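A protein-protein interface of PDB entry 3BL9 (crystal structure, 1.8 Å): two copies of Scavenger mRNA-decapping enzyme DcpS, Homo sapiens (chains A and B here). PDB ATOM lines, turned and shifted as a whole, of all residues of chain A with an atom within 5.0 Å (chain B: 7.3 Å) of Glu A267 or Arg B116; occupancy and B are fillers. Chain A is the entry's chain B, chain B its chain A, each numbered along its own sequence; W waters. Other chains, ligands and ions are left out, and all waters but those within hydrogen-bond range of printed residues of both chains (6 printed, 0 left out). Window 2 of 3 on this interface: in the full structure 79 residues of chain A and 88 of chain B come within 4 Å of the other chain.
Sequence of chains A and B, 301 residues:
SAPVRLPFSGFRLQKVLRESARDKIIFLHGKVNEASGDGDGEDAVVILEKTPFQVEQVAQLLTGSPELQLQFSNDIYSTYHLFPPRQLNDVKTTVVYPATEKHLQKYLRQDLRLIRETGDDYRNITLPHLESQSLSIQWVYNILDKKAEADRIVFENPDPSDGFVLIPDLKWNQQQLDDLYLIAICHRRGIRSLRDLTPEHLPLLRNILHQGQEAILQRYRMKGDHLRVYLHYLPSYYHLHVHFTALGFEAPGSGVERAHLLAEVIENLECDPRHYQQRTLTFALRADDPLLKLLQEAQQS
NH1 of Arg B116 lies within salt-bridge range of OE2 of Glu A267, at 2.8 Å.
The side-chain amide oxygen (OD1) of Asn A268 sits at hydrogen-bond distance from the guanidinium group (NH2) of Arg B279 (3.0 Å).
The side-chain sulfur (SG) of Cys A271 sits at hydrogen-bond distance from the guanidinium group (NH1) of Arg B279 (3.5 Å).
The guanidinium group of Arg B116 lies within hydrogen-bond range of the side-chain hydroxyl of Thr B282, 2.8 Å away.
The backbone carbonyl oxygen (O) of Arg B279 lies within hydrogen-bond range of the guanidinium group (NH1) of Arg B195 (2.9 Å).
The backbone carbonyl oxygen (O) of Glu A264 sits close to the side-chain amide nitrogen (ND2) of Asn A268 (3.4 Å).
The side-chain sulfur of Cys A271 is in hydrogen-bond range of the backbone carbonyl oxygen of Glu A267.
Among the printed residues, merely in contact across the chains: Glu A267 with Thr B280, Ala A263 with Arg B116 and Glu A267 with Arg B279.
Glu A267 touches just these residues of chain B: Arg B116, Arg B279 and Thr B280.
Printed residues of chain B within 4 Å of Asn A268: Arg B279.
Of chain A, only Ala A263 and Glu A267 come within 4 Å of Arg B116.
Glu B117 touches none of the printed residues of chain A.
Of the printed residues of chain A, Thr B280 touches Glu A267 (3.6 Å).
The nearest residue of chain A that does not touch Arg B116 is Glu A264 (4.04 Å).
Hydrophobic or aromatic side chains of chain A that line the printed part of chain B: Ala A263.
Among the printed residues, 6 pairs touch across the chains.
No position is printed for both chains.
Water W3 lies within hydrogen-bond range of the side-chain carboxylate (OE2) of Glu A264 (2.4 Å), the backbone carbonyl oxygen (O) of Thr B280 (2.7 Å), the side-chain hydroxyl (OG1) of Thr B282 (2.8 Å) and the guanidinium group (NH2) of Arg B116 (2.8 Å).
Water W2 lies within hydrogen-bond range of OE2 of Glu A264 (2.5 Å) and N of Thr B282 (2.8 Å).
Water W1 lies within hydrogen-bond range of OG1 of Thr B280 (2.6 Å) and OE2 of Glu A267 (2.8 Å).
Water W4 lies within hydrogen-bond range of the side-chain carboxylate (OE1) of Glu A267, the guanidinium group (NH2) of Arg B279 and the backbone carbonyl oxygen (O) of Thr B280.
Water W5 lies within hydrogen-bond range of NE of Arg B279 (2.8 Å), OE1 of Glu A267 (2.8 Å) and N of Thr B280 (3.0 Å).
Water W6 lies within hydrogen-bond range of OD2 of Asp A272 (3.0 Å), OD1 of Asn A268 (3.1 Å) and NH1 of Arg B279 (3.2 Å).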
ATOM      1  N   ALA A 263       2.458 -19.959  -6.642  1.00  0.00           N
ATOM      2  CA  ALA A 263       3.127 -19.286  -5.524  1.00  0.00           C
ATOM      3  C   ALA A 263       4.661 -19.466  -5.550  1.00  0.00           C
ATOM      4  O   ALA A 263       5.404 -18.553  -5.223  1.00  0.00           O
ATOM      5  CB  ALA A 263       2.548 -19.735  -4.170  1.00  0.00           C
ATOM      6  N   GLU A 264       5.143 -20.636  -5.938  1.00  0.00           N
ATOM      7  CA  GLU A 264       6.573 -20.869  -6.039  1.00  0.00           C
ATOM      8  C   GLU A 264       7.193 -20.231  -7.267  1.00  0.00           C
ATOM      9  O   GLU A 264       8.343 -19.803  -7.214  1.00  0.00           O
ATOM     10  CB  GLU A 264       6.906 -22.365  -6.000  1.00  0.00           C
ATOM     11  CG  GLU A 264       6.454 -23.027  -4.726  1.00  0.00           C
ATOM     12  CD  GLU A 264       7.030 -24.452  -4.560  1.00  0.00           C
ATOM     13  OE1 GLU A 264       7.460 -25.056  -5.571  1.00  0.00           O
ATOM     14  OE2 GLU A 264       7.014 -24.963  -3.428  1.00  0.00           O
ATOM     15  N   VAL A 265       6.452 -20.174  -8.377  1.00  0.00           N
ATOM     16  CA  VAL A 265       6.911 -19.466  -9.571  1.00  0.00           C
ATOM     17  C   VAL A 265       7.182 -17.993  -9.165  1.00  0.00           C
ATOM     18  O   VAL A 265       8.271 -17.450  -9.426  1.00  0.00           O
ATOM     19  CB  VAL A 265       5.888 -19.590 -10.765  1.00  0.00           C
ATOM     20  CG1 VAL A 265       6.255 -18.643 -11.933  1.00  0.00           C
ATOM     21  CG2 VAL A 265       5.804 -21.042 -11.288  1.00  0.00           C
ATOM     22  N   ILE A 266       6.220 -17.395  -8.467  1.00  0.00           N
ATOM     23  CA  ILE A 266       6.337 -15.996  -8.002  1.00  0.00           C
ATOM     24  C   ILE A 266       7.607 -15.829  -7.142  1.00  0.00           C
ATOM     25  O   ILE A 266       8.462 -14.963  -7.412  1.00  0.00           O
ATOM     26  CB  ILE A 266       5.044 -15.540  -7.278  1.00  0.00           C
ATOM     27  CG1 ILE A 266       3.895 -15.399  -8.284  1.00  0.00           C
ATOM     28  CG2 ILE A 266       5.245 -14.190  -6.491  1.00  0.00           C
ATOM     29  CD1 ILE A 266       2.549 -15.252  -7.636  1.00  0.00           C
ATOM     30  N   GLU A 267       7.784 -16.708  -6.155  1.00  0.00           N
ATOM     31  CA  GLU A 267       8.913 -16.580  -5.204  1.00  0.00           C
ATOM     32  C   GLU A 267      10.248 -16.863  -5.860  1.00  0.00           C
ATOM     33  O   GLU A 267      11.249 -16.217  -5.511  1.00  0.00           O
ATOM     34  CB  GLU A 267       8.670 -17.419  -3.948  1.00  0.00           C
ATOM     35  CG  GLU A 267       7.525 -16.864  -3.139  1.00  0.00           C
ATOM     36  CD  GLU A 267       7.174 -17.651  -1.901  1.00  0.00           C
ATOM     37  OE1 GLU A 267       7.788 -18.715  -1.668  1.00  0.00           O
ATOM     38  OE2 GLU A 267       6.258 -17.200  -1.166  1.00  0.00           O
ATOM     39  N   ASN A 268      10.279 -17.791  -6.827  1.00  0.00           N
ATOM     40  CA  ASN A 268      11.470 -17.981  -7.656  1.00  0.00           C
ATOM     41  C   ASN A 268      11.872 -16.694  -8.396  1.00  0.00           C
ATOM     42  O   ASN A 268      13.032 -16.283  -8.340  1.00  0.00           O
ATOM     43  CB  ASN A 268      11.297 -19.119  -8.665  1.00  0.00           C
ATOM     44  CG  ASN A 268      11.475 -20.499  -8.039  1.00  0.00           C
ATOM     45  OD1 ASN A 268      12.099 -20.632  -6.981  1.00  0.00           O
ATOM     46  ND2 ASN A 268      10.919 -21.536  -8.687  1.00  0.00           N
ATOM     47  N   LEU A 269      10.921 -16.071  -9.073  1.00  0.00           N
ATOM     48  CA  LEU A 269      11.181 -14.797  -9.771  1.00  0.00           C
ATOM     49  C   LEU A 269      11.641 -13.691  -8.813  1.00  0.00           C
ATOM     50  O   LEU A 269      12.473 -12.860  -9.175  1.00  0.00           O
ATOM     51  CB  LEU A 269       9.926 -14.325 -10.499  1.00  0.00           C
ATOM     52  CG  LEU A 269       9.587 -15.190 -11.713  1.00  0.00           C
ATOM     53  CD1 LEU A 269       8.245 -14.773 -12.299  1.00  0.00           C
ATOM     54  CD2 LEU A 269      10.702 -15.129 -12.753  1.00  0.00           C
ATOM     55  N   GLU A 270      11.108 -13.702  -7.600  1.00  0.00           N
ATOM     56  CA  GLU A 270      11.412 -12.665  -6.619  1.00  0.00           C
ATOM     57  C   GLU A 270      12.843 -12.767  -6.097  1.00  0.00           C
ATOM     58  O   GLU A 270      13.441 -11.765  -5.784  1.00  0.00           O
ATOM     59  CB  GLU A 270      10.429 -12.720  -5.470  1.00  0.00           C
ATOM     60  CG  GLU A 270       9.132 -12.093  -5.799  1.00  0.00           C
ATOM     61  CD  GLU A 270       8.118 -12.267  -4.748  1.00  0.00           C
ATOM     62  OE1 GLU A 270       8.311 -13.115  -3.871  1.00  0.00           O
ATOM     63  OE2 GLU A 270       7.121 -11.548  -4.790  1.00  0.00           O
ATOM     64  N   CYS A 271      13.395 -13.964  -6.008  1.00  0.00           N
ATOM     65  CA  CYS A 271      14.744 -14.111  -5.462  1.00  0.00           C
ATOM     66  C   CYS A 271      15.795 -14.542  -6.461  1.00  0.00           C
ATOM     67  O   CYS A 271      16.997 -14.509  -6.148  1.00  0.00           O
ATOM     68  CB  CYS A 271      14.744 -15.021  -4.252  1.00  0.00           C
ATOM     69  SG  CYS A 271      14.374 -16.726  -4.552  1.00  0.00           S
ATOM     70  N   ASP A 272      15.363 -14.853  -7.681  1.00  0.00           N
ATOM     71  CA  ASP A 272      16.215 -15.433  -8.685  1.00  0.00           C
ATOM     72  C   ASP A 272      15.629 -15.013 -10.042  1.00  0.00           C
ATOM     73  O   ASP A 272      14.965 -15.800 -10.705  1.00  0.00           O
ATOM     74  CB  ASP A 272      16.174 -16.947  -8.432  1.00  0.00           C
ATOM     75  CG  ASP A 272      17.058 -17.756  -9.324  1.00  0.00           C
ATOM     76  OD1 ASP A 272      17.954 -17.234 -10.038  1.00  0.00           O
ATOM     77  OD2 ASP A 272      16.836 -18.999  -9.298  1.00  0.00           O
ATOM     78  N   LEU B 114      -3.934 -27.008   2.278  1.00  0.00           N
ATOM     79  CA  LEU B 114      -2.565 -26.579   1.992  1.00  0.00           C
ATOM     80  C   LEU B 114      -2.066 -25.535   2.977  1.00  0.00           C
ATOM     81  O   LEU B 114      -2.829 -24.718   3.489  1.00  0.00           O
ATOM     82  CB  LEU B 114      -2.445 -25.967   0.590  1.00  0.00           C
ATOM     83  CG  LEU B 114      -2.527 -26.864  -0.623  1.00  0.00           C
ATOM     84  CD1 LEU B 114      -2.284 -26.009  -1.860  1.00  0.00           C
ATOM     85  CD2 LEU B 114      -1.511 -28.013  -0.490  1.00  0.00           C
ATOM     86  N   ILE B 115      -0.763 -25.535   3.190  1.00  0.00           N
ATOM     87  CA  ILE B 115      -0.118 -24.562   4.031  1.00  0.00           C
ATOM     88  C   ILE B 115       1.228 -24.238   3.382  1.00  0.00           C
ATOM     89  O   ILE B 115       1.856 -25.111   2.754  1.00  0.00           O
ATOM     90  CB  ILE B 115       0.030 -25.096   5.479  1.00  0.00           C
ATOM     91  CG1 ILE B 115       0.381 -23.980   6.473  1.00  0.00           C
ATOM     92  CG2 ILE B 115       1.061 -26.223   5.543  1.00  0.00           C
ATOM     93  CD1 ILE B 115      -0.845 -23.090   6.850  1.00  0.00           C
ATOM     94  N   ARG B 116       1.659 -22.982   3.533  1.00  0.00           N
ATOM     95  CA  ARG B 116       2.948 -22.529   3.041  1.00  0.00           C
ATOM     96  C   ARG B 116       3.833 -22.203   4.226  1.00  0.00           C
ATOM     97  O   ARG B 116       3.638 -21.177   4.889  1.00  0.00           O
ATOM     98  CB  ARG B 116       2.752 -21.309   2.139  1.00  0.00           C
ATOM     99  CG  ARG B 116       1.767 -21.626   1.036  1.00  0.00           C
ATOM    100  CD  ARG B 116       2.036 -20.885  -0.249  1.00  0.00           C
ATOM    101  NE  ARG B 116       3.335 -21.159  -0.862  1.00  0.00           N
ATOM    102  CZ  ARG B 116       4.323 -20.279  -1.027  1.00  0.00           C
ATOM    103  NH1 ARG B 116       4.192 -19.014  -0.630  1.00  0.00           N
ATOM    104  NH2 ARG B 116       5.451 -20.669  -1.601  1.00  0.00           N
ATOM    105  N   GLU B 117       4.805 -23.074   4.478  1.00  0.00           N
ATOM    106  CA  GLU B 117       5.698 -22.986   5.627  1.00  0.00           C
ATOM    107  C   GLU B 117       6.981 -22.230   5.261  1.00  0.00           C
ATOM    108  O   GLU B 117       7.812 -22.724   4.499  1.00  0.00           O
ATOM    109  CB  GLU B 117       6.017 -24.424   6.072  1.00  0.00           C
ATOM    110  CG  GLU B 117       6.875 -24.599   7.311  1.00  0.00           C
ATOM    111  CD  GLU B 117       7.457 -26.017   7.388  1.00  0.00           C
ATOM    112  OE1 GLU B 117       7.159 -26.724   8.357  1.00  0.00           O
ATOM    113  OE2 GLU B 117       8.195 -26.415   6.468  1.00  0.00           O
ATOM    114  N   THR B 118       7.152 -21.025   5.812  1.00  0.00           N
ATOM    115  CA  THR B 118       8.396 -20.290   5.631  1.00  0.00           C
ATOM    116  C   THR B 118       9.547 -20.964   6.391  1.00  0.00           C
ATOM    117  O   THR B 118       9.329 -21.841   7.217  1.00  0.00           O
ATOM    118  CB  THR B 118       8.249 -18.807   6.060  1.00  0.00           C
ATOM    119  OG1 THR B 118       8.098 -18.737   7.480  1.00  0.00           O
ATOM    120  CG2 THR B 118       7.051 -18.169   5.390  1.00  0.00           C
ATOM    121  N   GLY B 119      10.781 -20.573   6.092  1.00  0.00           N
ATOM    122  CA  GLY B 119      11.956 -21.110   6.809  1.00  0.00           C
ATOM    123  C   GLY B 119      11.871 -20.872   8.317  1.00  0.00           C
ATOM    124  O   GLY B 119      12.246 -21.732   9.106  1.00  0.00           O
ATOM    125  N   ASP B 121       8.909 -20.304   9.993  1.00  0.00           N
ATOM    126  CA  ASP B 121       7.799 -21.162  10.450  1.00  0.00           C
ATOM    127  C   ASP B 121       8.350 -22.534  10.812  1.00  0.00           C
ATOM    128  O   ASP B 121       7.988 -23.083  11.852  1.00  0.00           O
ATOM    129  CB  ASP B 121       6.732 -21.362   9.368  1.00  0.00           C
ATOM    130  CG  ASP B 121       5.903 -20.129   9.089  1.00  0.00           C
ATOM    131  OD1 ASP B 121       5.942 -19.155   9.889  1.00  0.00           O
ATOM    132  OD2 ASP B 121       5.192 -20.140   8.050  1.00  0.00           O
ATOM    133  N   ARG B 195      14.163 -30.375   4.972  1.00  0.00           N
ATOM    134  CA  ARG B 195      14.596 -29.255   5.817  1.00  0.00           C
ATOM    135  C   ARG B 195      15.970 -29.431   6.408  1.00  0.00           C
ATOM    136  O   ARG B 195      16.620 -28.445   6.739  1.00  0.00           O
ATOM    137  CB  ARG B 195      13.590 -29.035   6.944  1.00  0.00           C
ATOM    138  CG  ARG B 195      12.287 -28.404   6.497  1.00  0.00           C
ATOM    139  CD  ARG B 195      12.497 -27.010   5.991  1.00  0.00           C
ATOM    140  NE  ARG B 195      11.247 -26.305   5.785  1.00  0.00           N
ATOM    141  CZ  ARG B 195      11.135 -25.167   5.106  1.00  0.00           C
ATOM    142  NH1 ARG B 195      12.183 -24.618   4.517  1.00  0.00           N
ATOM    143  NH2 ARG B 195       9.952 -24.610   4.959  1.00  0.00           N
ATOM    144  N   ARG B 279      13.870 -21.315   2.085  1.00  0.00           N
ATOM    145  CA  ARG B 279      12.747 -21.166   1.157  1.00  0.00           C
ATOM    146  C   ARG B 279      11.441 -21.671   1.763  1.00  0.00           C
ATOM    147  O   ARG B 279      11.453 -22.536   2.625  1.00  0.00           O
ATOM    148  CB  ARG B 279      13.059 -21.852  -0.181  1.00  0.00           C
ATOM    149  CG  ARG B 279      14.205 -21.189  -0.977  1.00  0.00           C
ATOM    150  CD  ARG B 279      13.823 -19.758  -1.445  1.00  0.00           C
ATOM    151  NE  ARG B 279      12.600 -19.831  -2.225  1.00  0.00           N
ATOM    152  CZ  ARG B 279      12.531 -20.024  -3.544  1.00  0.00           C
ATOM    153  NH1 ARG B 279      13.631 -20.122  -4.280  1.00  0.00           N
ATOM    154  NH2 ARG B 279      11.326 -20.119  -4.129  1.00  0.00           N
ATOM    155  N   THR B 280      10.319 -21.110   1.301  1.00  0.00           N
ATOM    156  CA  THR B 280       9.007 -21.516   1.754  1.00  0.00           C
ATOM    157  C   THR B 280       8.617 -22.787   1.018  1.00  0.00           C
ATOM    158  O   THR B 280       8.719 -22.834  -0.191  1.00  0.00           O
ATOM    159  CB  THR B 280       7.957 -20.417   1.497  1.00  0.00           C
ATOM    160  OG1 THR B 280       8.334 -19.237   2.219  1.00  0.00           O
ATOM    161  CG2 THR B 280       6.556 -20.824   1.937  1.00  0.00           C
ATOM    162  N   LEU B 281       8.174 -23.792   1.768  1.00  0.00           N
ATOM    163  CA  LEU B 281       7.707 -25.072   1.218  1.00  0.00           C
ATOM    164  C   LEU B 281       6.190 -25.194   1.349  1.00  0.00           C
ATOM    165  O   LEU B 281       5.589 -24.776   2.350  1.00  0.00           O
ATOM    166  CB  LEU B 281       8.414 -26.238   1.922  1.00  0.00           C
ATOM    167  CG  LEU B 281       9.935 -26.289   1.837  1.00  0.00           C
ATOM    168  CD1 LEU B 281      10.503 -27.515   2.579  1.00  0.00           C
ATOM    169  CD2 LEU B 281      10.442 -26.261   0.396  1.00  0.00           C
ATOM    170  N   THR B 282       5.558 -25.747   0.320  1.00  0.00           N
ATOM    171  CA  THR B 282       4.105 -25.890   0.284  1.00  0.00           C
ATOM    172  C   THR B 282       3.700 -27.368   0.390  1.00  0.00           C
ATOM    173  O   THR B 282       4.207 -28.210  -0.355  1.00  0.00           O
ATOM    174  CB  THR B 282       3.528 -25.296  -1.004  1.00  0.00           C
ATOM    175  OG1 THR B 282       3.922 -23.915  -1.108  1.00  0.00           O
ATOM    176  CG2 THR B 282       2.015 -25.394  -1.006  1.00  0.00           C
ATOM    177  N   PHE B 283       2.812 -27.661   1.329  1.00  0.00           N
ATOM    178  CA  PHE B 283       2.319 -29.013   1.538  1.00  0.00           C
ATOM    179  C   PHE B 283       0.933 -29.038   2.177  1.00  0.00           C
ATOM    180  O   PHE B 283       0.467 -28.029   2.764  1.00  0.00           O
ATOM    181  CB  PHE B 283       3.304 -29.803   2.425  1.00  0.00           C
ATOM    182  CG  PHE B 283       3.586 -29.142   3.756  1.00  0.00           C
ATOM    183  CD1 PHE B 283       2.825 -29.440   4.867  1.00  0.00           C
ATOM    184  CD2 PHE B 283       4.638 -28.247   3.883  1.00  0.00           C
ATOM    185  CE1 PHE B 283       3.113 -28.859   6.101  1.00  0.00           C
ATOM    186  CE2 PHE B 283       4.922 -27.638   5.110  1.00  0.00           C
ATOM    187  CZ  PHE B 283       4.155 -27.953   6.216  1.00  0.00           C
ATOM    188  N   LEU B 295       0.571 -23.505  12.562  1.00  0.00           N
ATOM    189  CA  LEU B 295       1.080 -22.727  11.425  1.00  0.00           C
ATOM    190  C   LEU B 295       0.133 -21.596  11.020  1.00  0.00           C
ATOM    191  O   LEU B 295       0.574 -20.469  10.806  1.00  0.00           O
ATOM    192  CB  LEU B 295       1.361 -23.634  10.211  1.00  0.00           C
ATOM    193  CG  LEU B 295       2.576 -24.567  10.344  1.00  0.00           C
ATOM    194  CD1 LEU B 295       2.700 -25.529   9.156  1.00  0.00           C
ATOM    195  CD2 LEU B 295       3.862 -23.780  10.487  1.00  0.00           C
HETATM  196  O   HOH W   1       7.075 -17.085   1.539  1.00  0.00           O
HETATM  197  O   HOH W   2       7.022 -26.847  -1.852  1.00  0.00           O
HETATM  198  O   HOH W   3       6.585 -23.275  -1.737  1.00  0.00           O
HETATM  199  O   HOH W   4       9.079 -20.938  -2.624  1.00  0.00           O
HETATM  200  O   HOH W   5      10.443 -18.885  -0.689  1.00  0.00           O
HETATM  201  O   HOH W   6      15.150 -19.967  -7.051  1.00  0.00           O
